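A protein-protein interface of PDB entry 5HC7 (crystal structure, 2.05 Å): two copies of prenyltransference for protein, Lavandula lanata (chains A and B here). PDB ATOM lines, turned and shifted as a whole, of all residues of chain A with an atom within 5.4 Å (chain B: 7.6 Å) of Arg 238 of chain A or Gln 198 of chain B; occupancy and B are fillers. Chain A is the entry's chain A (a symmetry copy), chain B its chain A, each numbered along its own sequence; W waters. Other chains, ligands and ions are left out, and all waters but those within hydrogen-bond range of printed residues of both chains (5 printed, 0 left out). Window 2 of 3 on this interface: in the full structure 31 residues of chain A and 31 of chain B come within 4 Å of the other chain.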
ATOM      1  N   GLN A 198       5.386 -10.066   9.901  1.00  0.00           N
ATOM      2  CA  GLN A 198       5.702 -11.212  10.768  1.00  0.00           C
ATOM      3  C   GLN A 198       6.594 -12.179  10.002  1.00  0.00           C
ATOM      4  O   GLN A 198       6.149 -13.204   9.460  1.00  0.00           O
ATOM      5  CB  GLN A 198       4.416 -11.841  11.259  1.00  0.00           C
ATOM      6  CG  GLN A 198       3.666 -10.977  12.295  1.00  0.00           C
ATOM      7  CD  GLN A 198       2.299 -11.612  12.602  1.00  0.00           C
ATOM      8  OE1 GLN A 198       1.343 -11.426  11.852  1.00  0.00           O
ATOM      9  NE2 GLN A 198       2.270 -12.485  13.501  1.00  0.00           N
ATOM     10  N   THR A 211      14.707 -17.322  20.963  1.00  0.00           N
ATOM     11  CA  THR A 211      14.225 -15.948  20.989  1.00  0.00           C
ATOM     12  C   THR A 211      12.708 -15.731  21.002  1.00  0.00           C
ATOM     13  O   THR A 211      11.950 -16.377  20.261  1.00  0.00           O
ATOM     14  CB  THR A 211      14.768 -15.255  19.760  1.00  0.00           C
ATOM     15  OG1 THR A 211      16.172 -15.489  19.776  1.00  0.00           O
ATOM     16  CG2 THR A 211      14.449 -13.780  19.755  1.00  0.00           C
ATOM     17  N   GLU A 212      12.271 -14.864  21.917  1.00  0.00           N
ATOM     18  CA  GLU A 212      10.874 -14.409  21.958  1.00  0.00           C
ATOM     19  C   GLU A 212      10.691 -13.344  20.905  1.00  0.00           C
ATOM     20  O   GLU A 212      11.459 -12.397  20.857  1.00  0.00           O
ATOM     21  CB  GLU A 212      10.523 -13.780  23.320  1.00  0.00           C
ATOM     22  CG  GLU A 212      10.472 -14.795  24.439  1.00  0.00           C
ATOM     23  CD  GLU A 212       9.326 -15.798  24.239  1.00  0.00           C
ATOM     24  OE1 GLU A 212       8.258 -15.444  23.707  1.00  0.00           O
ATOM     25  OE2 GLU A 212       9.481 -16.944  24.601  1.00  0.00           O
ATOM     26  N   PHE A 213       9.658 -13.496  20.085  1.00  0.00           N
ATOM     27  CA  PHE A 213       9.333 -12.540  19.060  1.00  0.00           C
ATOM     28  C   PHE A 213       8.263 -11.580  19.535  1.00  0.00           C
ATOM     29  O   PHE A 213       7.276 -11.969  20.177  1.00  0.00           O
ATOM     30  CB  PHE A 213       8.816 -13.249  17.801  1.00  0.00           C
ATOM     31  CG  PHE A 213       9.830 -14.139  17.135  1.00  0.00           C
ATOM     32  CD1 PHE A 213      11.165 -13.965  17.333  1.00  0.00           C
ATOM     33  CD2 PHE A 213       9.419 -15.219  16.431  1.00  0.00           C
ATOM     34  CE1 PHE A 213      12.095 -14.808  16.718  1.00  0.00           C
ATOM     35  CE2 PHE A 213      10.318 -16.051  15.794  1.00  0.00           C
ATOM     36  CZ  PHE A 213      11.661 -15.840  15.910  1.00  0.00           C
ATOM     37  N   TYR A 214       8.441 -10.325  19.165  1.00  0.00           N
ATOM     38  CA  TYR A 214       7.501  -9.295  19.444  1.00  0.00           C
ATOM     39  C   TYR A 214       7.288  -8.456  18.241  1.00  0.00           C
ATOM     40  O   TYR A 214       8.192  -7.769  17.776  1.00  0.00           O
ATOM     41  CB  TYR A 214       8.024  -8.446  20.602  1.00  0.00           C
ATOM     42  CG  TYR A 214       7.130  -7.262  20.994  1.00  0.00           C
ATOM     43  CD1 TYR A 214       6.058  -7.421  21.895  1.00  0.00           C
ATOM     44  CD2 TYR A 214       7.323  -6.006  20.411  1.00  0.00           C
ATOM     45  CE1 TYR A 214       5.247  -6.319  22.237  1.00  0.00           C
ATOM     46  CE2 TYR A 214       6.543  -4.918  20.715  1.00  0.00           C
ATOM     47  CZ  TYR A 214       5.524  -5.072  21.635  1.00  0.00           C
ATOM     48  OH  TYR A 214       4.807  -3.996  21.928  1.00  0.00           O
ATOM     49  N   PHE A 215       6.052  -8.459  17.779  1.00  0.00           N
ATOM     50  CA  PHE A 215       5.655  -7.709  16.588  1.00  0.00           C
ATOM     51  C   PHE A 215       4.756  -6.571  16.958  1.00  0.00           C
ATOM     52  O   PHE A 215       3.801  -6.792  17.663  1.00  0.00           O
ATOM     53  CB  PHE A 215       4.899  -8.643  15.660  1.00  0.00           C
ATOM     54  CG  PHE A 215       5.710  -9.836  15.272  1.00  0.00           C
ATOM     55  CD1 PHE A 215       6.727  -9.732  14.311  1.00  0.00           C
ATOM     56  CD2 PHE A 215       5.518 -11.062  15.916  1.00  0.00           C
ATOM     57  CE1 PHE A 215       7.504 -10.828  13.993  1.00  0.00           C
ATOM     58  CE2 PHE A 215       6.282 -12.161  15.572  1.00  0.00           C
ATOM     59  CZ  PHE A 215       7.294 -12.036  14.627  1.00  0.00           C
ATOM     60  N   SER A 234       5.863  -7.186  27.499  1.00  0.00           N
ATOM     61  CA  SER A 234       5.459  -8.469  26.856  1.00  0.00           C
ATOM     62  C   SER A 234       6.441  -9.587  27.190  1.00  0.00           C
ATOM     63  O   SER A 234       6.064 -10.694  27.596  1.00  0.00           O
ATOM     64  CB  SER A 234       5.284  -8.278  25.356  1.00  0.00           C
ATOM     65  OG  SER A 234       4.854  -9.454  24.651  1.00  0.00           O
ATOM     66  N   TYR A 235       7.729  -9.290  27.079  1.00  0.00           N
ATOM     67  CA  TYR A 235       8.735 -10.287  27.327  1.00  0.00           C
ATOM     68  C   TYR A 235       8.576 -10.844  28.765  1.00  0.00           C
ATOM     69  O   TYR A 235       8.579 -12.056  28.969  1.00  0.00           O
ATOM     70  CB  TYR A 235      10.124  -9.699  27.114  1.00  0.00           C
ATOM     71  CG  TYR A 235      11.246 -10.648  27.443  1.00  0.00           C
ATOM     72  CD1 TYR A 235      11.604 -11.632  26.561  1.00  0.00           C
ATOM     73  CD2 TYR A 235      11.940 -10.575  28.690  1.00  0.00           C
ATOM     74  CE1 TYR A 235      12.623 -12.522  26.853  1.00  0.00           C
ATOM     75  CE2 TYR A 235      12.955 -11.473  29.010  1.00  0.00           C
ATOM     76  CZ  TYR A 235      13.292 -12.436  28.079  1.00  0.00           C
ATOM     77  OH  TYR A 235      14.301 -13.315  28.332  1.00  0.00           O
ATOM     78  N   ARG A 236       8.414  -9.948  29.738  1.00  0.00           N
ATOM     79  CA  ARG A 236       8.334 -10.344  31.140  1.00  0.00           C
ATOM     80  C   ARG A 236       7.075 -11.202  31.381  1.00  0.00           C
ATOM     81  O   ARG A 236       7.110 -12.177  32.141  1.00  0.00           O
ATOM     82  CB  ARG A 236       8.415  -9.107  32.064  1.00  0.00           C
ATOM     83  CG  ARG A 236       9.740  -8.340  32.020  1.00  0.00           C
ATOM     84  CD  ARG A 236       9.865  -7.182  33.049  1.00  0.00           C
ATOM     85  NE  ARG A 236       9.535  -5.822  32.528  1.00  0.00           N
ATOM     86  CZ  ARG A 236       8.417  -5.095  32.778  1.00  0.00           C
ATOM     87  NH1 ARG A 236       7.414  -5.524  33.562  1.00  0.00           N
ATOM     88  NH2 ARG A 236       8.287  -3.904  32.223  1.00  0.00           N
ATOM     89  N   CYS A 237       5.976 -10.887  30.716  1.00  0.00           N
ATOM     90  CA  CYS A 237       4.826 -11.791  30.699  1.00  0.00           C
ATOM     91  C   CYS A 237       4.994 -13.201  30.062  1.00  0.00           C
ATOM     92  O   CYS A 237       4.160 -14.026  30.265  1.00  0.00           O
ATOM     93  CB  CYS A 237       3.631 -11.087  30.050  1.00  0.00           C
ATOM     94  SG  CYS A 237       2.976  -9.859  31.192  1.00  0.00           S
ATOM     95  N   ARG A 238       6.036 -13.522  29.317  1.00  0.00           N
ATOM     96  CA  ARG A 238       6.079 -14.856  28.714  1.00  0.00           C
ATOM     97  C   ARG A 238       6.682 -15.899  29.705  1.00  0.00           C
ATOM     98  O   ARG A 238       7.293 -15.485  30.710  1.00  0.00           O
ATOM     99  CB  ARG A 238       6.853 -14.830  27.401  1.00  0.00           C
ATOM    100  CG  ARG A 238       6.784 -13.508  26.622  1.00  0.00           C
ATOM    101  CD  ARG A 238       6.129 -13.753  25.327  1.00  0.00           C
ATOM    102  NE  ARG A 238       5.853 -12.596  24.485  1.00  0.00           N
ATOM    103  CZ  ARG A 238       6.222 -12.466  23.202  1.00  0.00           C
ATOM    104  NH1 ARG A 238       6.981 -13.390  22.578  1.00  0.00           N
ATOM    105  NH2 ARG A 238       5.817 -11.410  22.514  1.00  0.00           N
ATOM    106  N   ASP B  21       1.629 -27.515  19.567  1.00  0.00           N
ATOM    107  CA  ASP B  21       1.912 -27.089  20.913  1.00  0.00           C
ATOM    108  C   ASP B  21       0.567 -26.941  21.636  1.00  0.00           C
ATOM    109  O   ASP B  21      -0.457 -26.914  20.994  1.00  0.00           O
ATOM    110  CB  ASP B  21       2.676 -25.738  20.885  1.00  0.00           C
ATOM    111  CG  ASP B  21       3.404 -25.390  22.217  1.00  0.00           C
ATOM    112  OD1 ASP B  21       3.635 -26.314  22.988  1.00  0.00           O
ATOM    113  OD2 ASP B  21       3.766 -24.209  22.523  1.00  0.00           O
ATOM    114  N   ARG B 193       2.189 -21.654  14.104  1.00  0.00           N
ATOM    115  CA  ARG B 193       2.453 -22.161  15.460  1.00  0.00           C
ATOM    116  C   ARG B 193       1.208 -21.974  16.318  1.00  0.00           C
ATOM    117  O   ARG B 193       0.755 -20.876  16.514  1.00  0.00           O
ATOM    118  CB  ARG B 193       3.631 -21.453  16.127  1.00  0.00           C
ATOM    119  CG  ARG B 193       3.902 -22.054  17.482  1.00  0.00           C
ATOM    120  CD  ARG B 193       5.150 -21.585  18.164  1.00  0.00           C
ATOM    121  NE  ARG B 193       5.183 -22.230  19.457  1.00  0.00           N
ATOM    122  CZ  ARG B 193       6.250 -22.703  20.064  1.00  0.00           C
ATOM    123  NH1 ARG B 193       7.472 -22.650  19.541  1.00  0.00           N
ATOM    124  NH2 ARG B 193       6.069 -23.272  21.229  1.00  0.00           N
ATOM    125  N   ALA B 194       0.694 -23.085  16.810  1.00  0.00           N
ATOM    126  CA  ALA B 194      -0.446 -23.127  17.723  1.00  0.00           C
ATOM    127  C   ALA B 194       0.004 -22.865  19.158  1.00  0.00           C
ATOM    128  O   ALA B 194       1.187 -23.036  19.514  1.00  0.00           O
ATOM    129  CB  ALA B 194      -1.109 -24.468  17.637  1.00  0.00           C
ATOM    130  N   ALA B 195      -0.991 -22.495  19.947  1.00  0.00           N
ATOM    131  CA  ALA B 195      -0.957 -22.369  21.369  1.00  0.00           C
ATOM    132  C   ALA B 195      -0.352 -21.034  21.821  1.00  0.00           C
ATOM    133  O   ALA B 195      -0.015 -20.844  22.968  1.00  0.00           O
ATOM    134  CB  ALA B 195      -0.271 -23.580  22.014  1.00  0.00           C
ATOM    135  N   GLY B 196      -0.152 -20.106  20.922  1.00  0.00           N
ATOM    136  CA  GLY B 196       0.104 -18.743  21.414  1.00  0.00           C
ATOM    137  C   GLY B 196       1.557 -18.308  21.615  1.00  0.00           C
ATOM    138  O   GLY B 196       1.785 -17.133  21.709  1.00  0.00           O
ATOM    139  N   GLU B 197       2.539 -19.223  21.720  1.00  0.00           N
ATOM    140  CA  GLU B 197       3.891 -18.786  21.922  1.00  0.00           C
ATOM    141  C   GLU B 197       4.423 -18.252  20.597  1.00  0.00           C
ATOM    142  O   GLU B 197       4.047 -18.716  19.489  1.00  0.00           O
ATOM    143  CB  GLU B 197       4.793 -19.911  22.440  1.00  0.00           C
ATOM    144  CG  GLU B 197       4.265 -20.605  23.677  1.00  0.00           C
ATOM    145  CD  GLU B 197       4.172 -19.663  24.875  1.00  0.00           C
ATOM    146  OE1 GLU B 197       3.318 -19.917  25.704  1.00  0.00           O
ATOM    147  OE2 GLU B 197       4.914 -18.685  25.033  1.00  0.00           O
ATOM    148  N   GLN B 198       5.301 -17.273  20.733  1.00  0.00           N
ATOM    149  CA  GLN B 198       5.882 -16.562  19.583  1.00  0.00           C
ATOM    150  C   GLN B 198       7.392 -16.759  19.593  1.00  0.00           C
ATOM    151  O   GLN B 198       8.170 -15.896  20.031  1.00  0.00           O
ATOM    152  CB  GLN B 198       5.466 -15.108  19.628  1.00  0.00           C
ATOM    153  CG  GLN B 198       3.976 -14.885  19.297  1.00  0.00           C
ATOM    154  CD  GLN B 198       3.609 -13.410  19.536  1.00  0.00           C
ATOM    155  OE1 GLN B 198       3.350 -13.007  20.668  1.00  0.00           O
ATOM    156  NE2 GLN B 198       3.805 -12.618  18.584  1.00  0.00           N
ATOM    157  N   ARG B 199       7.760 -17.965  19.196  1.00  0.00           N
ATOM    158  CA  ARG B 199       9.152 -18.365  19.115  1.00  0.00           C
ATOM    159  C   ARG B 199       9.201 -19.656  18.275  1.00  0.00           C
ATOM    160  O   ARG B 199       8.168 -20.270  18.016  1.00  0.00           O
ATOM    161  CB  ARG B 199       9.724 -18.548  20.531  1.00  0.00           C
ATOM    162  CG  ARG B 199       8.885 -19.510  21.391  1.00  0.00           C
ATOM    163  CD  ARG B 199       9.572 -19.812  22.712  1.00  0.00           C
ATOM    164  NE  ARG B 199       8.792 -20.744  23.544  1.00  0.00           N
ATOM    165  CZ  ARG B 199       7.971 -20.402  24.540  1.00  0.00           C
ATOM    166  NH1 ARG B 199       7.808 -19.135  24.908  1.00  0.00           N
ATOM    167  NH2 ARG B 199       7.297 -21.366  25.170  1.00  0.00           N
ATOM    168  N   LEU B 200      10.417 -20.024  17.858  1.00  0.00           N
ATOM    169  CA  LEU B 200      10.712 -21.126  16.965  1.00  0.00           C
ATOM    170  C   LEU B 200      11.065 -22.390  17.713  1.00  0.00           C
ATOM    171  O   LEU B 200      10.861 -23.479  17.193  1.00  0.00           O
ATOM    172  CB  LEU B 200      11.880 -20.759  16.007  1.00  0.00           C
ATOM    173  CG  LEU B 200      11.651 -19.534  15.137  1.00  0.00           C
ATOM    174  CD1 LEU B 200      12.873 -19.254  14.298  1.00  0.00           C
ATOM    175  CD2 LEU B 200      10.386 -19.723  14.243  1.00  0.00           C
ATOM    176  N   SER B 201      11.524 -22.260  18.939  1.00  0.00           N
ATOM    177  CA  SER B 201      11.820 -23.403  19.784  1.00  0.00           C
ATOM    178  C   SER B 201      12.763 -24.398  19.125  1.00  0.00           C
ATOM    179  O   SER B 201      12.673 -25.589  19.372  1.00  0.00           O
ATOM    180  CB  SER B 201      10.543 -24.137  20.301  1.00  0.00           C
ATOM    181  OG  SER B 201       9.672 -23.266  21.014  1.00  0.00           O
ATOM    182  N   TYR B 214       2.643 -17.206  11.343  1.00  0.00           N
ATOM    183  CA  TYR B 214       1.294 -17.126  11.785  1.00  0.00           C
ATOM    184  C   TYR B 214       1.145 -17.790  13.102  1.00  0.00           C
ATOM    185  O   TYR B 214       1.316 -18.999  13.229  1.00  0.00           O
ATOM    186  CB  TYR B 214       0.392 -17.791  10.746  1.00  0.00           C
ATOM    187  CG  TYR B 214      -1.100 -17.818  11.105  1.00  0.00           C
ATOM    188  CD1 TYR B 214      -1.945 -16.731  10.807  1.00  0.00           C
ATOM    189  CD2 TYR B 214      -1.642 -18.906  11.798  1.00  0.00           C
ATOM    190  CE1 TYR B 214      -3.312 -16.776  11.151  1.00  0.00           C
ATOM    191  CE2 TYR B 214      -2.965 -18.974  12.156  1.00  0.00           C
ATOM    192  CZ  TYR B 214      -3.796 -17.923  11.818  1.00  0.00           C
ATOM    193  OH  TYR B 214      -5.074 -18.032  12.154  1.00  0.00           O
ATOM    194  N   PHE B 215       0.748 -16.996  14.078  1.00  0.00           N
ATOM    195  CA  PHE B 215       0.567 -17.464  15.451  1.00  0.00           C
ATOM    196  C   PHE B 215      -0.883 -17.463  15.820  1.00  0.00           C
ATOM    197  O   PHE B 215      -1.532 -16.466  15.620  1.00  0.00           O
ATOM    198  CB  PHE B 215       1.307 -16.523  16.384  1.00  0.00           C
ATOM    199  CG  PHE B 215       2.762 -16.428  16.059  1.00  0.00           C
ATOM    200  CD1 PHE B 215       3.647 -17.455  16.422  1.00  0.00           C
ATOM    201  CD2 PHE B 215       3.253 -15.348  15.321  1.00  0.00           C
ATOM    202  CE1 PHE B 215       4.981 -17.383  16.075  1.00  0.00           C
ATOM    203  CE2 PHE B 215       4.596 -15.270  15.002  1.00  0.00           C
ATOM    204  CZ  PHE B 215       5.456 -16.302  15.357  1.00  0.00           C
ATOM    205  N   THR B 216      -1.402 -18.580  16.314  1.00  0.00           N
ATOM    206  CA  THR B 216      -2.763 -18.624  16.818  1.00  0.00           C
ATOM    207  C   THR B 216      -2.694 -19.037  18.238  1.00  0.00           C
ATOM    208  O   THR B 216      -1.958 -20.016  18.556  1.00  0.00           O
ATOM    209  CB  THR B 216      -3.617 -19.857  16.445  1.00  0.00           C
ATOM    210  OG1 THR B 216      -3.149 -20.551  15.318  1.00  0.00           O
ATOM    211  CG2 THR B 216      -4.999 -19.531  16.394  1.00  0.00           C
HETATM  212  O   HOH W   1       2.855  -9.903  22.035  1.00  0.00           O
HETATM  213  O   HOH W   2       4.051  -9.879  19.343  1.00  0.00           O
HETATM  214  O   HOH W   3      12.564 -18.362  18.626  1.00  0.00           O
HETATM  215  O   HOH W   4       0.044 -14.264  13.365  1.00  0.00           O
HETATM  216  O   HOH W   5       5.934 -16.636  23.423  1.00  0.00           O
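Gln 198 of chain A touches Phe 215 of chain B, and with the chains exchanged Phe 215 of chain A touches Gln 198 of chain B. Phe 215 of chain B touches its own counterpart, Phe 215 of chain A. Positions printed for both chains: 198, 214 and 215. Of the 10 pairs that touch across the chains among the printed residues, 3 have their exchanged pair printed and touching as well.
The backbone carbonyl oxygen (O) of Gln 198 of chain B is in hydrogen-bond range of the backbone NH (N) of Phe 213 of chain A, 2.8 Å away. OE1 of Gln 198 of chain B is in hydrogen-bond range of NH2 of Arg 238 of chain A (3.5 Å). The guanidinium group of Arg 199 of chain B lies within salt-bridge range of the side-chain carboxylate of Glu 212 of chain A (2.8 Å).
The backbone carbonyl oxygen (O) of Arg 199 of chain B sits at hydrogen-bond distance from the guanidinium group (NH1) of Arg 193 of chain B. NH1 of Arg 199 of chain B is in salt-bridge range of OE2 of Glu 197 of chain B, 2.9 Å away. The side-chain carboxylate (OE1) of Glu 212 of chain A lies within salt-bridge range of the guanidinium group (NH1) of Arg 238 of chain A, at 2.7 Å. NH1 of Arg 238 of chain A is in hydrogen-bond range of O of Phe 213 of chain A (2.8 Å). OG of Ser 234 of chain A is in hydrogen-bond range of NH2 of Arg 238 of chain A.
Among the printed residues, pairs that only touch across the chains: Thr 211 of chain A with Arg 199 of chain B (3.1 Å), Phe 215 of chain A with Gln 198 of chain B (3.5 Å), Gln 198 of chain A with Phe 215 of chain B (3.5 Å), Phe 215 of chain A with Phe 215 of chain B (3.6 Å), Glu 212 of chain A with Gln 198 of chain B (3.6 Å), Phe 213 of chain A with Leu 200 of chain B (3.8 Å) and Thr 211 of chain A with Gln 198 of chain B (3.8 Å).
Water W5 lies within hydrogen-bond range of OE1 of Glu 212 of chain A (2.6 Å), OE2 of Glu 197 of chain B (2.8 Å), N of Gln 198 of chain B (2.8 Å) and NH1 of Arg 199 of chain B (3.5 Å). Water W3 bridges O of Thr 211 of chain A (2.6 Å) and N of Leu 200 of chain B (2.8 Å). Water W2 bridges the side-chain amide nitrogen (NE2) of Gln 198 of chain B (2.9 Å) and the backbone NH (N) of Phe 215 of chain A (2.9 Å). Water W4 bridges the side-chain amide nitrogen (NE2) of Gln 198 of chain A (2.9 Å) and the backbone NH (N) of Phe 215 of chain B (2.9 Å). Water W1 lies within hydrogen-bond range of OG of Ser 234 of chain A (3.3 Å), NH2 of Arg 238 of chain A (3.4 Å) and OE1 of Gln 198 of chain B (3.4 Å).
Of the printed residues of chain B, Glu 212 of chain A touches Gln 198 and Arg 199. Of the printed residues of chain B, Phe 215 of chain A touches Gln 198 (3.5 Å) and Phe 215 (3.6 Å). Of chain B, only Gln 198 comes within 4 Å of Arg 238 of chain A. Asp 21 of chain B touches none of the printed residues of chain A. Gln 198 of chain B touches five residues of chain A. Of the printed residues of chain A, Arg 199 of chain B touches Thr 211 (3.1 Å) and Glu 212 (2.8 Å). Printed residues of chain A within 4 Å of Leu 200 of chain B: Phe 213. Of the printed residues of chain A, Phe 215 of chain B touches Gln 198 and Phe 215. The nearest residue of chain B that does not touch Arg 238 of chain A is Glu 197 of chain B (4.9 Å). The nearest residue of chain A that does not touch Gln 198 of chain B is Tyr 214 of chain A (5.0 Å). The nearest printed residue of chain A that does not touch Leu 200 of chain B is Thr 211 of chain A (4.6 Å).
Printed residues of chain B that touch a printed residue of chain A: Gln 198, Arg 199, Leu 200 and Phe 215. Hydrophobic or aromatic side chains of chain B within 4 Å of the printed part of chain A: Leu 200 and Phe 215. Printed residues of chain A that touch a printed residue of chain B: Gln 198, Thr 211, Glu 212, Phe 213, Phe 215 and Arg 238. Hydrophobic or aromatic side chains of chain A within 4 Å of the printed part of chain B: Phe 213 and Phe 215. Among the printed residues, 10 pairs touch across the chains.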
